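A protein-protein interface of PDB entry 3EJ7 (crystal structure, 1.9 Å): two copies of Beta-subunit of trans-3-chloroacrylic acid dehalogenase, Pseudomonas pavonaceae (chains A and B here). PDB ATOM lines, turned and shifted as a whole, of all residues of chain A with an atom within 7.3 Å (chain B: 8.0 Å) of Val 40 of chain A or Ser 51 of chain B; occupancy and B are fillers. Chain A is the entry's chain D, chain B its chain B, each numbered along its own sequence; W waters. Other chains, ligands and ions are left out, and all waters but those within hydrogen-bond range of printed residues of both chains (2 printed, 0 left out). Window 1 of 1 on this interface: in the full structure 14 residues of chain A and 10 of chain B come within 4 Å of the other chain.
The side-chain amide nitrogen (ND2) of Asn 49 of chain B sits at hydrogen-bond distance from the backbone carbonyl oxygen (O) of Leu 42 of chain A, at 2.7 Å. N of Ser 51 of chain B sits at hydrogen-bond distance from O of Val 40 of chain A, 2.8 Å away. O of Ile 38 of chain A is in hydrogen-bond range of N of Ser 53 of chain B (3.3 Å). The backbone NH (N) of Ser 53 of chain B sits at hydrogen-bond distance from the side-chain amide oxygen (OD1) of Asn 39 of chain A (3.2 Å). The backbone NH (N) of Gly 54 of chain B lies within hydrogen-bond range of the backbone carbonyl oxygen (O) of Pro 35 of chain A (2.9 Å). The backbone NH (N) of Gly 54 of chain B is in hydrogen-bond range of the backbone carbonyl oxygen (O) of Ile 38 of chain A (2.9 Å). The backbone carbonyl oxygen (O) of Pro 35 of chain A sits close to the backbone carbonyl oxygen (O) of Ser 53 of chain B (3.2 Å).
The side-chain hydroxyl of Ser 51 of chain B sits at hydrogen-bond distance from the backbone carbonyl oxygen of Arg 55 of chain B. The backbone carbonyl oxygen (O) of Pro 1 of chain A is in hydrogen-bond range of the backbone NH (N) of Asn 39 of chain A, at 2.9 Å. The backbone carbonyl oxygen (O) of Asn 39 of chain A is in hydrogen-bond range of the backbone NH (N) of Ile 3 of chain A (2.8 Å). The backbone NH of Leu 41 of chain A lies within hydrogen-bond range of the backbone carbonyl oxygen of Ile 3 of chain A, 2.9 Å away. The backbone NH of Cys 5 of chain A lies within hydrogen-bond range of the backbone carbonyl oxygen of Leu 41 of chain A (2.8 Å). ND2 of Asn 39 of chain A sits at hydrogen-bond distance from O of Ile 37 of chain A, at 3.2 Å.
Ile 20 of chain A touches Ala 48 of chain B. Ser 51 of chain B touches Ile 20 of chain A. Ile 20 of chain A touches Ile 56 of chain B. Arg 21 of chain A touches Ile 56 of chain B. Ser 51 of chain B touches Asn 39 of chain A. OD1 of Asn 39 of chain A touches CA of Ile 52 of chain B (3.7 Å). O of Val 40 of chain A touches O of Asn 49 of chain B (3.9 Å). Val 40 of chain A touches Met 50 of chain B. Leu 41 of chain A touches Asn 49 of chain B. Leu 41 of chain A touches Met 50 of chain B.
Val 23 of chain A touches none of the printed residues of chain B. Of chain B, only Asn 49, Met 50 and Ser 51 come within 4 Å of Val 40 of chain A. Of the printed residues of chain A, Ala 48 of chain B touches Ile 20 (3.4 Å). Ser 51 of chain B touches four residues of chain A. Of the printed residues of chain A, Ile 56 of chain B touches Ile 20 and Arg 21. The nearest residue of chain B that does not touch Val 40 of chain A is Ile 52 of chain B (5.1 Å). The nearest printed residue of chain A that does not touch Gly 54 of chain B is Asn 39 of chain A (5.1 Å).
Printed residues of chain A that touch a printed residue of chain B: Ile 20, Arg 21, Ile 24, Pro 35, Ile 38, Asn 39, Val 40, Leu 41 and Leu 42. Hydrophobic or aromatic side chains of chain A that line the printed part of chain B: Ile 20, Ile 24, Val 40, Leu 41 and Leu 42. Hydrophobic or aromatic side chains of chain B that line the printed part of chain A: Met 50, Ile 52 and Ile 56. Among the printed residues, 19 pairs touch across the chains. Among the printed residues, no Asp or Glu carboxylate lies within 4 Å of a Lys or Arg side-chain nitrogen of the other chain.
No position is printed for both chains. Of the 19 pairs that touch across the chains among the printed residues, none has its exchanged pair printed and touching as well.
Water W1 lies within hydrogen-bond range of OG of Ser 53 of chain B (2.9 Å) and ND2 of Asn 39 of chain A (3.3 Å). Water W2 lies within hydrogen-bond range of the backbone carbonyl oxygen of Leu 42 of chain A (2.9 Å) and the side-chain amide nitrogen of Asn 49 of chain B (3.5 Å).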
ATOM      1  N   PRO A   1     -12.073  29.330  27.259  1.00  0.00           N
ATOM      2  CA  PRO A   1     -12.209  30.293  26.178  1.00  0.00           C
ATOM      3  C   PRO A   1     -12.598  29.610  24.851  1.00  0.00           C
ATOM      4  O   PRO A   1     -12.525  28.368  24.741  1.00  0.00           O
ATOM      5  CB  PRO A   1     -10.801  30.876  26.052  1.00  0.00           C
ATOM      6  CG  PRO A   1     -10.202  30.736  27.402  1.00  0.00           C
ATOM      7  CD  PRO A   1     -10.829  29.523  28.036  1.00  0.00           C
ATOM      8  N   PHE A   2     -13.009  30.403  23.865  1.00  0.00           N
ATOM      9  CA  PHE A   2     -13.244  29.868  22.517  1.00  0.00           C
ATOM     10  C   PHE A   2     -12.482  30.757  21.551  1.00  0.00           C
ATOM     11  O   PHE A   2     -12.768  31.943  21.480  1.00  0.00           O
ATOM     12  CB  PHE A   2     -14.732  29.862  22.189  1.00  0.00           C
ATOM     13  CG  PHE A   2     -15.056  29.533  20.765  1.00  0.00           C
ATOM     14  CD1 PHE A   2     -14.327  28.581  20.074  1.00  0.00           C
ATOM     15  CD2 PHE A   2     -16.166  30.113  20.142  1.00  0.00           C
ATOM     16  CE1 PHE A   2     -14.629  28.263  18.772  1.00  0.00           C
ATOM     17  CE2 PHE A   2     -16.496  29.784  18.807  1.00  0.00           C
ATOM     18  CZ  PHE A   2     -15.696  28.866  18.125  1.00  0.00           C
ATOM     19  N   ILE A   3     -11.475  30.190  20.884  1.00  0.00           N
ATOM     20  CA  ILE A   3     -10.647  30.931  19.923  1.00  0.00           C
ATOM     21  C   ILE A   3     -11.087  30.457  18.522  1.00  0.00           C
ATOM     22  O   ILE A   3     -11.030  29.248  18.187  1.00  0.00           O
ATOM     23  CB  ILE A   3      -9.115  30.733  20.113  1.00  0.00           C
ATOM     24  CG1 ILE A   3      -8.629  31.121  21.519  1.00  0.00           C
ATOM     25  CG2 ILE A   3      -8.314  31.568  19.077  1.00  0.00           C
ATOM     26  CD1 ILE A   3      -8.626  29.964  22.497  1.00  0.00           C
ATOM     27  N   GLU A   4     -11.555  31.391  17.713  1.00  0.00           N
ATOM     28  CA  GLU A   4     -11.953  31.034  16.345  1.00  0.00           C
ATOM     29  C   GLU A   4     -10.956  31.728  15.413  1.00  0.00           C
ATOM     30  O   GLU A   4     -10.774  32.947  15.505  1.00  0.00           O
ATOM     31  CB  GLU A   4     -13.390  31.456  16.049  1.00  0.00           C
ATOM     32  CG  GLU A   4     -13.827  31.206  14.597  1.00  0.00           C
ATOM     33  CD  GLU A   4     -15.317  31.421  14.369  1.00  0.00           C
ATOM     34  OE1 GLU A   4     -15.811  31.090  13.263  1.00  0.00           O
ATOM     35  OE2 GLU A   4     -16.003  31.913  15.276  1.00  0.00           O
ATOM     36  N   CYS A   5     -10.294  30.955  14.559  1.00  0.00           N
ATOM     37  CA  CYS A   5      -9.273  31.482  13.618  1.00  0.00           C
ATOM     38  C   CYS A   5      -9.716  31.329  12.166  1.00  0.00           C
ATOM     39  O   CYS A   5      -9.946  30.219  11.669  1.00  0.00           O
ATOM     40  CB  CYS A   5      -7.938  30.777  13.792  1.00  0.00           C
ATOM     41  SG  CYS A   5      -7.420  30.660  15.460  1.00  0.00           S
ATOM     42  N   LEU A  19      -0.807  24.173  14.406  1.00  0.00           N
ATOM     43  CA  LEU A  19      -1.353  25.499  14.693  1.00  0.00           C
ATOM     44  C   LEU A  19      -2.361  25.458  15.845  1.00  0.00           C
ATOM     45  O   LEU A  19      -2.317  26.327  16.737  1.00  0.00           O
ATOM     46  CB  LEU A  19      -1.995  26.122  13.435  1.00  0.00           C
ATOM     47  CG  LEU A  19      -2.775  27.430  13.627  1.00  0.00           C
ATOM     48  CD1 LEU A  19      -1.899  28.550  14.226  1.00  0.00           C
ATOM     49  CD2 LEU A  19      -3.407  27.858  12.322  1.00  0.00           C
ATOM     50  N   ILE A  20      -3.239  24.447  15.843  1.00  0.00           N
ATOM     51  CA  ILE A  20      -4.213  24.273  16.926  1.00  0.00           C
ATOM     52  C   ILE A  20      -3.481  23.941  18.241  1.00  0.00           C
ATOM     53  O   ILE A  20      -3.830  24.476  19.292  1.00  0.00           O
ATOM     54  CB  ILE A  20      -5.278  23.212  16.594  1.00  0.00           C
ATOM     55  CG1 ILE A  20      -6.135  23.684  15.407  1.00  0.00           C
ATOM     56  CG2 ILE A  20      -6.201  22.963  17.806  1.00  0.00           C
ATOM     57  CD1 ILE A  20      -6.902  22.568  14.681  1.00  0.00           C
ATOM     58  N   ARG A  21      -2.448  23.102  18.170  1.00  0.00           N
ATOM     59  CA  ARG A  21      -1.625  22.787  19.340  1.00  0.00           C
ATOM     60  C   ARG A  21      -0.966  24.048  19.913  1.00  0.00           C
ATOM     61  O   ARG A  21      -0.938  24.259  21.143  1.00  0.00           O
ATOM     62  CB  ARG A  21      -0.546  21.774  18.930  1.00  0.00           C
ATOM     63  CG  ARG A  21      -0.188  20.782  19.994  1.00  0.00           C
ATOM     64  CD  ARG A  21       0.832  19.758  19.480  1.00  0.00           C
ATOM     65  NE  ARG A  21       0.316  18.918  18.395  1.00  0.00           N
ATOM     66  CZ  ARG A  21      -0.460  17.851  18.565  1.00  0.00           C
ATOM     67  NH1 ARG A  21      -0.851  17.145  17.521  1.00  0.00           N
ATOM     68  NH2 ARG A  21      -0.852  17.486  19.778  1.00  0.00           N
ATOM     69  N   VAL A  23      -1.942  27.308  19.398  1.00  0.00           N
ATOM     70  CA  VAL A  23      -3.031  28.175  19.933  1.00  0.00           C
ATOM     71  C   VAL A  23      -3.401  27.779  21.365  1.00  0.00           C
ATOM     72  O   VAL A  23      -3.542  28.637  22.224  1.00  0.00           O
ATOM     73  CB  VAL A  23      -4.338  28.218  19.039  1.00  0.00           C
ATOM     74  CG1 VAL A  23      -5.542  28.836  19.811  1.00  0.00           C
ATOM     75  CG2 VAL A  23      -4.103  28.978  17.743  1.00  0.00           C
ATOM     76  N   ILE A  24      -3.566  26.482  21.605  1.00  0.00           N
ATOM     77  CA  ILE A  24      -3.893  25.977  22.950  1.00  0.00           C
ATOM     78  C   ILE A  24      -2.799  26.328  23.943  1.00  0.00           C
ATOM     79  O   ILE A  24      -3.107  26.911  24.991  1.00  0.00           O
ATOM     80  CB  ILE A  24      -4.212  24.453  22.974  1.00  0.00           C
ATOM     81  CG1 ILE A  24      -5.493  24.162  22.193  1.00  0.00           C
ATOM     82  CG2 ILE A  24      -4.357  23.966  24.422  1.00  0.00           C
ATOM     83  CD1 ILE A  24      -5.601  22.693  21.695  1.00  0.00           C
ATOM     84  N   THR A  27      -2.612  30.039  24.775  1.00  0.00           N
ATOM     85  CA  THR A  27      -3.756  30.500  25.547  1.00  0.00           C
ATOM     86  C   THR A  27      -3.548  30.123  26.995  1.00  0.00           C
ATOM     87  O   THR A  27      -3.717  30.952  27.880  1.00  0.00           O
ATOM     88  CB  THR A  27      -5.083  29.942  24.969  1.00  0.00           C
ATOM     89  OG1 THR A  27      -5.231  30.407  23.620  1.00  0.00           O
ATOM     90  CG2 THR A  27      -6.303  30.387  25.792  1.00  0.00           C
ATOM     91  N   PRO A  35      -6.275  23.755  29.706  1.00  0.00           N
ATOM     92  CA  PRO A  35      -6.562  23.226  28.374  1.00  0.00           C
ATOM     93  C   PRO A  35      -7.934  22.565  28.284  1.00  0.00           C
ATOM     94  O   PRO A  35      -8.527  22.543  27.212  1.00  0.00           O
ATOM     95  CB  PRO A  35      -5.442  22.211  28.136  1.00  0.00           C
ATOM     96  CG  PRO A  35      -4.692  22.121  29.442  1.00  0.00           C
ATOM     97  CD  PRO A  35      -4.916  23.395  30.139  1.00  0.00           C
ATOM     98  N   ILE A  37     -10.717  23.746  29.377  1.00  0.00           N
ATOM     99  CA  ILE A  37     -11.738  24.749  28.997  1.00  0.00           C
ATOM    100  C   ILE A  37     -11.357  25.541  27.734  1.00  0.00           C
ATOM    101  O   ILE A  37     -12.067  26.483  27.374  1.00  0.00           O
ATOM    102  CB  ILE A  37     -12.126  25.721  30.167  1.00  0.00           C
ATOM    103  CG1 ILE A  37     -10.884  26.443  30.701  1.00  0.00           C
ATOM    104  CG2 ILE A  37     -12.854  24.980  31.310  1.00  0.00           C
ATOM    105  CD1 ILE A  37     -11.179  27.771  31.369  1.00  0.00           C
ATOM    106  N   ILE A  38     -10.264  25.162  27.058  1.00  0.00           N
ATOM    107  CA  ILE A  38      -9.813  25.854  25.806  1.00  0.00           C
ATOM    108  C   ILE A  38     -10.414  25.175  24.568  1.00  0.00           C
ATOM    109  O   ILE A  38     -10.229  23.961  24.329  1.00  0.00           O
ATOM    110  CB  ILE A  38      -8.249  25.967  25.682  1.00  0.00           C
ATOM    111  CG1 ILE A  38      -7.667  26.742  26.866  1.00  0.00           C
ATOM    112  CG2 ILE A  38      -7.858  26.635  24.328  1.00  0.00           C
ATOM    113  CD1 ILE A  38      -6.113  26.760  26.950  1.00  0.00           C
ATOM    114  N   ASN A  39     -11.173  25.934  23.798  1.00  0.00           N
ATOM    115  CA  ASN A  39     -11.824  25.389  22.593  1.00  0.00           C
ATOM    116  C   ASN A  39     -11.373  26.181  21.381  1.00  0.00           C
ATOM    117  O   ASN A  39     -11.291  27.413  21.435  1.00  0.00           O
ATOM    118  CB  ASN A  39     -13.326  25.424  22.749  1.00  0.00           C
ATOM    119  CG  ASN A  39     -13.811  24.631  23.979  1.00  0.00           C
ATOM    120  OD1 ASN A  39     -14.081  23.420  23.897  1.00  0.00           O
ATOM    121  ND2 ASN A  39     -13.945  25.322  25.105  1.00  0.00           N
ATOM    122  N   VAL A  40     -11.027  25.470  20.308  1.00  0.00           N
ATOM    123  CA  VAL A  40     -10.423  26.102  19.133  1.00  0.00           C
ATOM    124  C   VAL A  40     -11.194  25.680  17.856  1.00  0.00           C
ATOM    125  O   VAL A  40     -11.517  24.484  17.636  1.00  0.00           O
ATOM    126  CB  VAL A  40      -8.919  25.788  18.992  1.00  0.00           C
ATOM    127  CG1 VAL A  40      -8.324  26.572  17.790  1.00  0.00           C
ATOM    128  CG2 VAL A  40      -8.133  26.139  20.252  1.00  0.00           C
ATOM    129  N   LEU A  41     -11.510  26.671  17.041  1.00  0.00           N
ATOM    130  CA  LEU A  41     -12.112  26.418  15.741  1.00  0.00           C
ATOM    131  C   LEU A  41     -11.273  27.073  14.642  1.00  0.00           C
ATOM    132  O   LEU A  41     -11.079  28.310  14.633  1.00  0.00           O
ATOM    133  CB  LEU A  41     -13.522  26.969  15.717  1.00  0.00           C
ATOM    134  CG  LEU A  41     -14.639  26.404  14.819  1.00  0.00           C
ATOM    135  CD1 LEU A  41     -15.416  27.506  14.114  1.00  0.00           C
ATOM    136  CD2 LEU A  41     -14.193  25.293  13.855  1.00  0.00           C
ATOM    137  N   LEU A  42     -10.765  26.239  13.733  1.00  0.00           N
ATOM    138  CA  LEU A  42      -9.990  26.728  12.595  1.00  0.00           C
ATOM    139  C   LEU A  42     -10.852  26.674  11.344  1.00  0.00           C
ATOM    140  O   LEU A  42     -11.363  25.606  10.983  1.00  0.00           O
ATOM    141  CB  LEU A  42      -8.717  25.904  12.454  1.00  0.00           C
ATOM    142  CG  LEU A  42      -7.646  26.264  11.444  1.00  0.00           C
ATOM    143  CD1 LEU A  42      -7.260  27.775  11.488  1.00  0.00           C
ATOM    144  CD2 LEU A  42      -6.427  25.381  11.760  1.00  0.00           C
ATOM    145  N   ALA B  46     -14.763  19.851   9.536  1.00  0.00           N
ATOM    146  CA  ALA B  46     -14.048  18.577   9.677  1.00  0.00           C
ATOM    147  C   ALA B  46     -13.563  18.536  11.114  1.00  0.00           C
ATOM    148  O   ALA B  46     -13.243  19.564  11.699  1.00  0.00           O
ATOM    149  CB  ALA B  46     -12.895  18.479   8.718  1.00  0.00           C
ATOM    150  N   GLU B  47     -13.552  17.332  11.677  1.00  0.00           N
ATOM    151  CA  GLU B  47     -13.076  17.094  13.022  1.00  0.00           C
ATOM    152  C   GLU B  47     -11.682  17.607  13.236  1.00  0.00           C
ATOM    153  O   GLU B  47     -11.391  18.126  14.315  1.00  0.00           O
ATOM    154  CB  GLU B  47     -13.100  15.606  13.326  1.00  0.00           C
ATOM    155  CG  GLU B  47     -14.459  15.035  13.192  1.00  0.00           C
ATOM    156  CD  GLU B  47     -15.167  14.900  14.518  1.00  0.00           C
ATOM    157  OE1 GLU B  47     -15.538  13.757  14.852  1.00  0.00           O
ATOM    158  OE2 GLU B  47     -15.341  15.922  15.224  1.00  0.00           O
ATOM    159  N   ALA B  48     -10.828  17.496  12.213  1.00  0.00           N
ATOM    160  CA  ALA B  48      -9.445  17.997  12.324  1.00  0.00           C
ATOM    161  C   ALA B  48      -9.370  19.509  12.555  1.00  0.00           C
ATOM    162  O   ALA B  48      -8.401  19.972  13.140  1.00  0.00           O
ATOM    163  CB  ALA B  48      -8.628  17.616  11.113  1.00  0.00           C
ATOM    164  N   ASN B  49     -10.389  20.261  12.135  1.00  0.00           N
ATOM    165  CA  ASN B  49     -10.414  21.735  12.322  1.00  0.00           C
ATOM    166  C   ASN B  49     -10.903  22.255  13.669  1.00  0.00           C
ATOM    167  O   ASN B  49     -10.953  23.486  13.882  1.00  0.00           O
ATOM    168  CB  ASN B  49     -11.184  22.430  11.193  1.00  0.00           C
ATOM    169  CG  ASN B  49     -10.342  22.544   9.922  1.00  0.00           C
ATOM    170  OD1 ASN B  49      -9.661  21.614   9.552  1.00  0.00           O
ATOM    171  ND2 ASN B  49     -10.375  23.684   9.286  1.00  0.00           N
ATOM    172  N   MET B  50     -11.282  21.334  14.559  1.00  0.00           N
ATOM    173  CA  MET B  50     -11.847  21.688  15.882  1.00  0.00           C
ATOM    174  C   MET B  50     -11.027  21.050  16.996  1.00  0.00           C
ATOM    175  O   MET B  50     -10.567  19.920  16.865  1.00  0.00           O
ATOM    176  CB  MET B  50     -13.295  21.247  15.998  1.00  0.00           C
ATOM    177  CG  MET B  50     -14.232  21.881  14.943  1.00  0.00           C
ATOM    178  SD  MET B  50     -15.972  21.562  15.170  1.00  0.00           S
ATOM    179  CE  MET B  50     -16.043  19.898  14.576  1.00  0.00           C
ATOM    180  N   SER B  51     -10.823  21.804  18.071  1.00  0.00           N
ATOM    181  CA  SER B  51     -10.257  21.277  19.301  1.00  0.00           C
ATOM    182  C   SER B  51     -11.301  21.513  20.380  1.00  0.00           C
ATOM    183  O   SER B  51     -11.591  22.669  20.710  1.00  0.00           O
ATOM    184  CB  SER B  51      -8.968  22.019  19.699  1.00  0.00           C
ATOM    185  OG  SER B  51      -8.422  21.480  20.902  1.00  0.00           O
ATOM    186  N   ILE B  52     -11.878  20.426  20.901  1.00  0.00           N
ATOM    187  CA  ILE B  52     -12.738  20.500  22.098  1.00  0.00           C
ATOM    188  C   ILE B  52     -11.877  20.247  23.337  1.00  0.00           C
ATOM    189  O   ILE B  52     -11.177  19.239  23.403  1.00  0.00           O
ATOM    190  CB  ILE B  52     -13.895  19.427  22.111  1.00  0.00           C
ATOM    191  CG1 ILE B  52     -14.492  19.145  20.709  1.00  0.00           C
ATOM    192  CG2 ILE B  52     -14.928  19.752  23.232  1.00  0.00           C
ATOM    193  CD1 ILE B  52     -14.708  20.339  19.811  1.00  0.00           C
ATOM    194  N   SER B  53     -11.915  21.163  24.310  1.00  0.00           N
ATOM    195  CA  SER B  53     -11.187  20.980  25.574  1.00  0.00           C
ATOM    196  C   SER B  53      -9.693  20.611  25.406  1.00  0.00           C
ATOM    197  O   SER B  53      -9.187  19.668  26.044  1.00  0.00           O
ATOM    198  CB  SER B  53     -11.911  19.925  26.441  1.00  0.00           C
ATOM    199  OG  SER B  53     -13.269  20.303  26.698  1.00  0.00           O
ATOM    200  N   GLY B  54      -8.997  21.357  24.554  1.00  0.00           N
ATOM    201  CA  GLY B  54      -7.566  21.182  24.343  1.00  0.00           C
ATOM    202  C   GLY B  54      -7.151  19.883  23.670  1.00  0.00           C
ATOM    203  O   GLY B  54      -5.967  19.588  23.596  1.00  0.00           O
ATOM    204  N   ARG B  55      -8.123  19.133  23.152  1.00  0.00           N
ATOM    205  CA  ARG B  55      -7.866  17.834  22.532  1.00  0.00           C
ATOM    206  C   ARG B  55      -7.623  17.983  21.043  1.00  0.00           C
ATOM    207  O   ARG B  55      -8.284  18.759  20.361  1.00  0.00           O
ATOM    208  CB  ARG B  55      -9.031  16.867  22.769  1.00  0.00           C
ATOM    209  CG  ARG B  55      -9.278  16.528  24.244  1.00  0.00           C
ATOM    210  CD  ARG B  55     -10.192  15.324  24.404  1.00  0.00           C
ATOM    211  NE  ARG B  55     -11.521  15.602  23.843  1.00  0.00           N
ATOM    212  CZ  ARG B  55     -12.570  15.984  24.566  1.00  0.00           C
ATOM    213  NH1 ARG B  55     -13.731  16.226  23.975  1.00  0.00           N
ATOM    214  NH2 ARG B  55     -12.452  16.123  25.883  1.00  0.00           N
ATOM    215  N   ILE B  56      -6.680  17.209  20.542  1.00  0.00           N
ATOM    216  CA  ILE B  56      -6.391  17.191  19.126  1.00  0.00           C
ATOM    217  C   ILE B  56      -6.980  15.909  18.547  1.00  0.00           C
ATOM    218  O   ILE B  56      -6.660  14.802  19.004  1.00  0.00           O
ATOM    219  CB  ILE B  56      -4.853  17.255  18.858  1.00  0.00           C
ATOM    220  CG1 ILE B  56      -4.250  18.549  19.438  1.00  0.00           C
ATOM    221  CG2 ILE B  56      -4.546  17.141  17.373  1.00  0.00           C
ATOM    222  CD1 ILE B  56      -4.584  19.814  18.633  1.00  0.00           C
ATOM    223  N   HIS B  57      -7.828  16.072  17.536  1.00  0.00           N
ATOM    224  CA  HIS B  57      -8.489  14.958  16.875  1.00  0.00           C
ATOM    225  C   HIS B  57      -7.510  13.918  16.308  1.00  0.00           C
ATOM    226  O   HIS B  57      -6.436  14.265  15.818  1.00  0.00           O
ATOM    227  CB  HIS B  57      -9.390  15.483  15.761  1.00  0.00           C
ATOM    228  CG  HIS B  57     -10.143  14.410  15.044  1.00  0.00           C
ATOM    229  ND1 HIS B  57     -11.094  13.629  15.666  1.00  0.00           N
ATOM    230  CD2 HIS B  57     -10.080  13.980  13.763  1.00  0.00           C
ATOM    231  CE1 HIS B  57     -11.598  12.773  14.793  1.00  0.00           C
ATOM    232  NE2 HIS B  57     -10.999  12.964  13.631  1.00  0.00           N
HETATM  233  O   HOH W   1     -14.400  22.879  27.209  1.00  0.00           O
HETATM  234  O   HOH W   2     -13.701  24.649   9.465  1.00  0.00           O
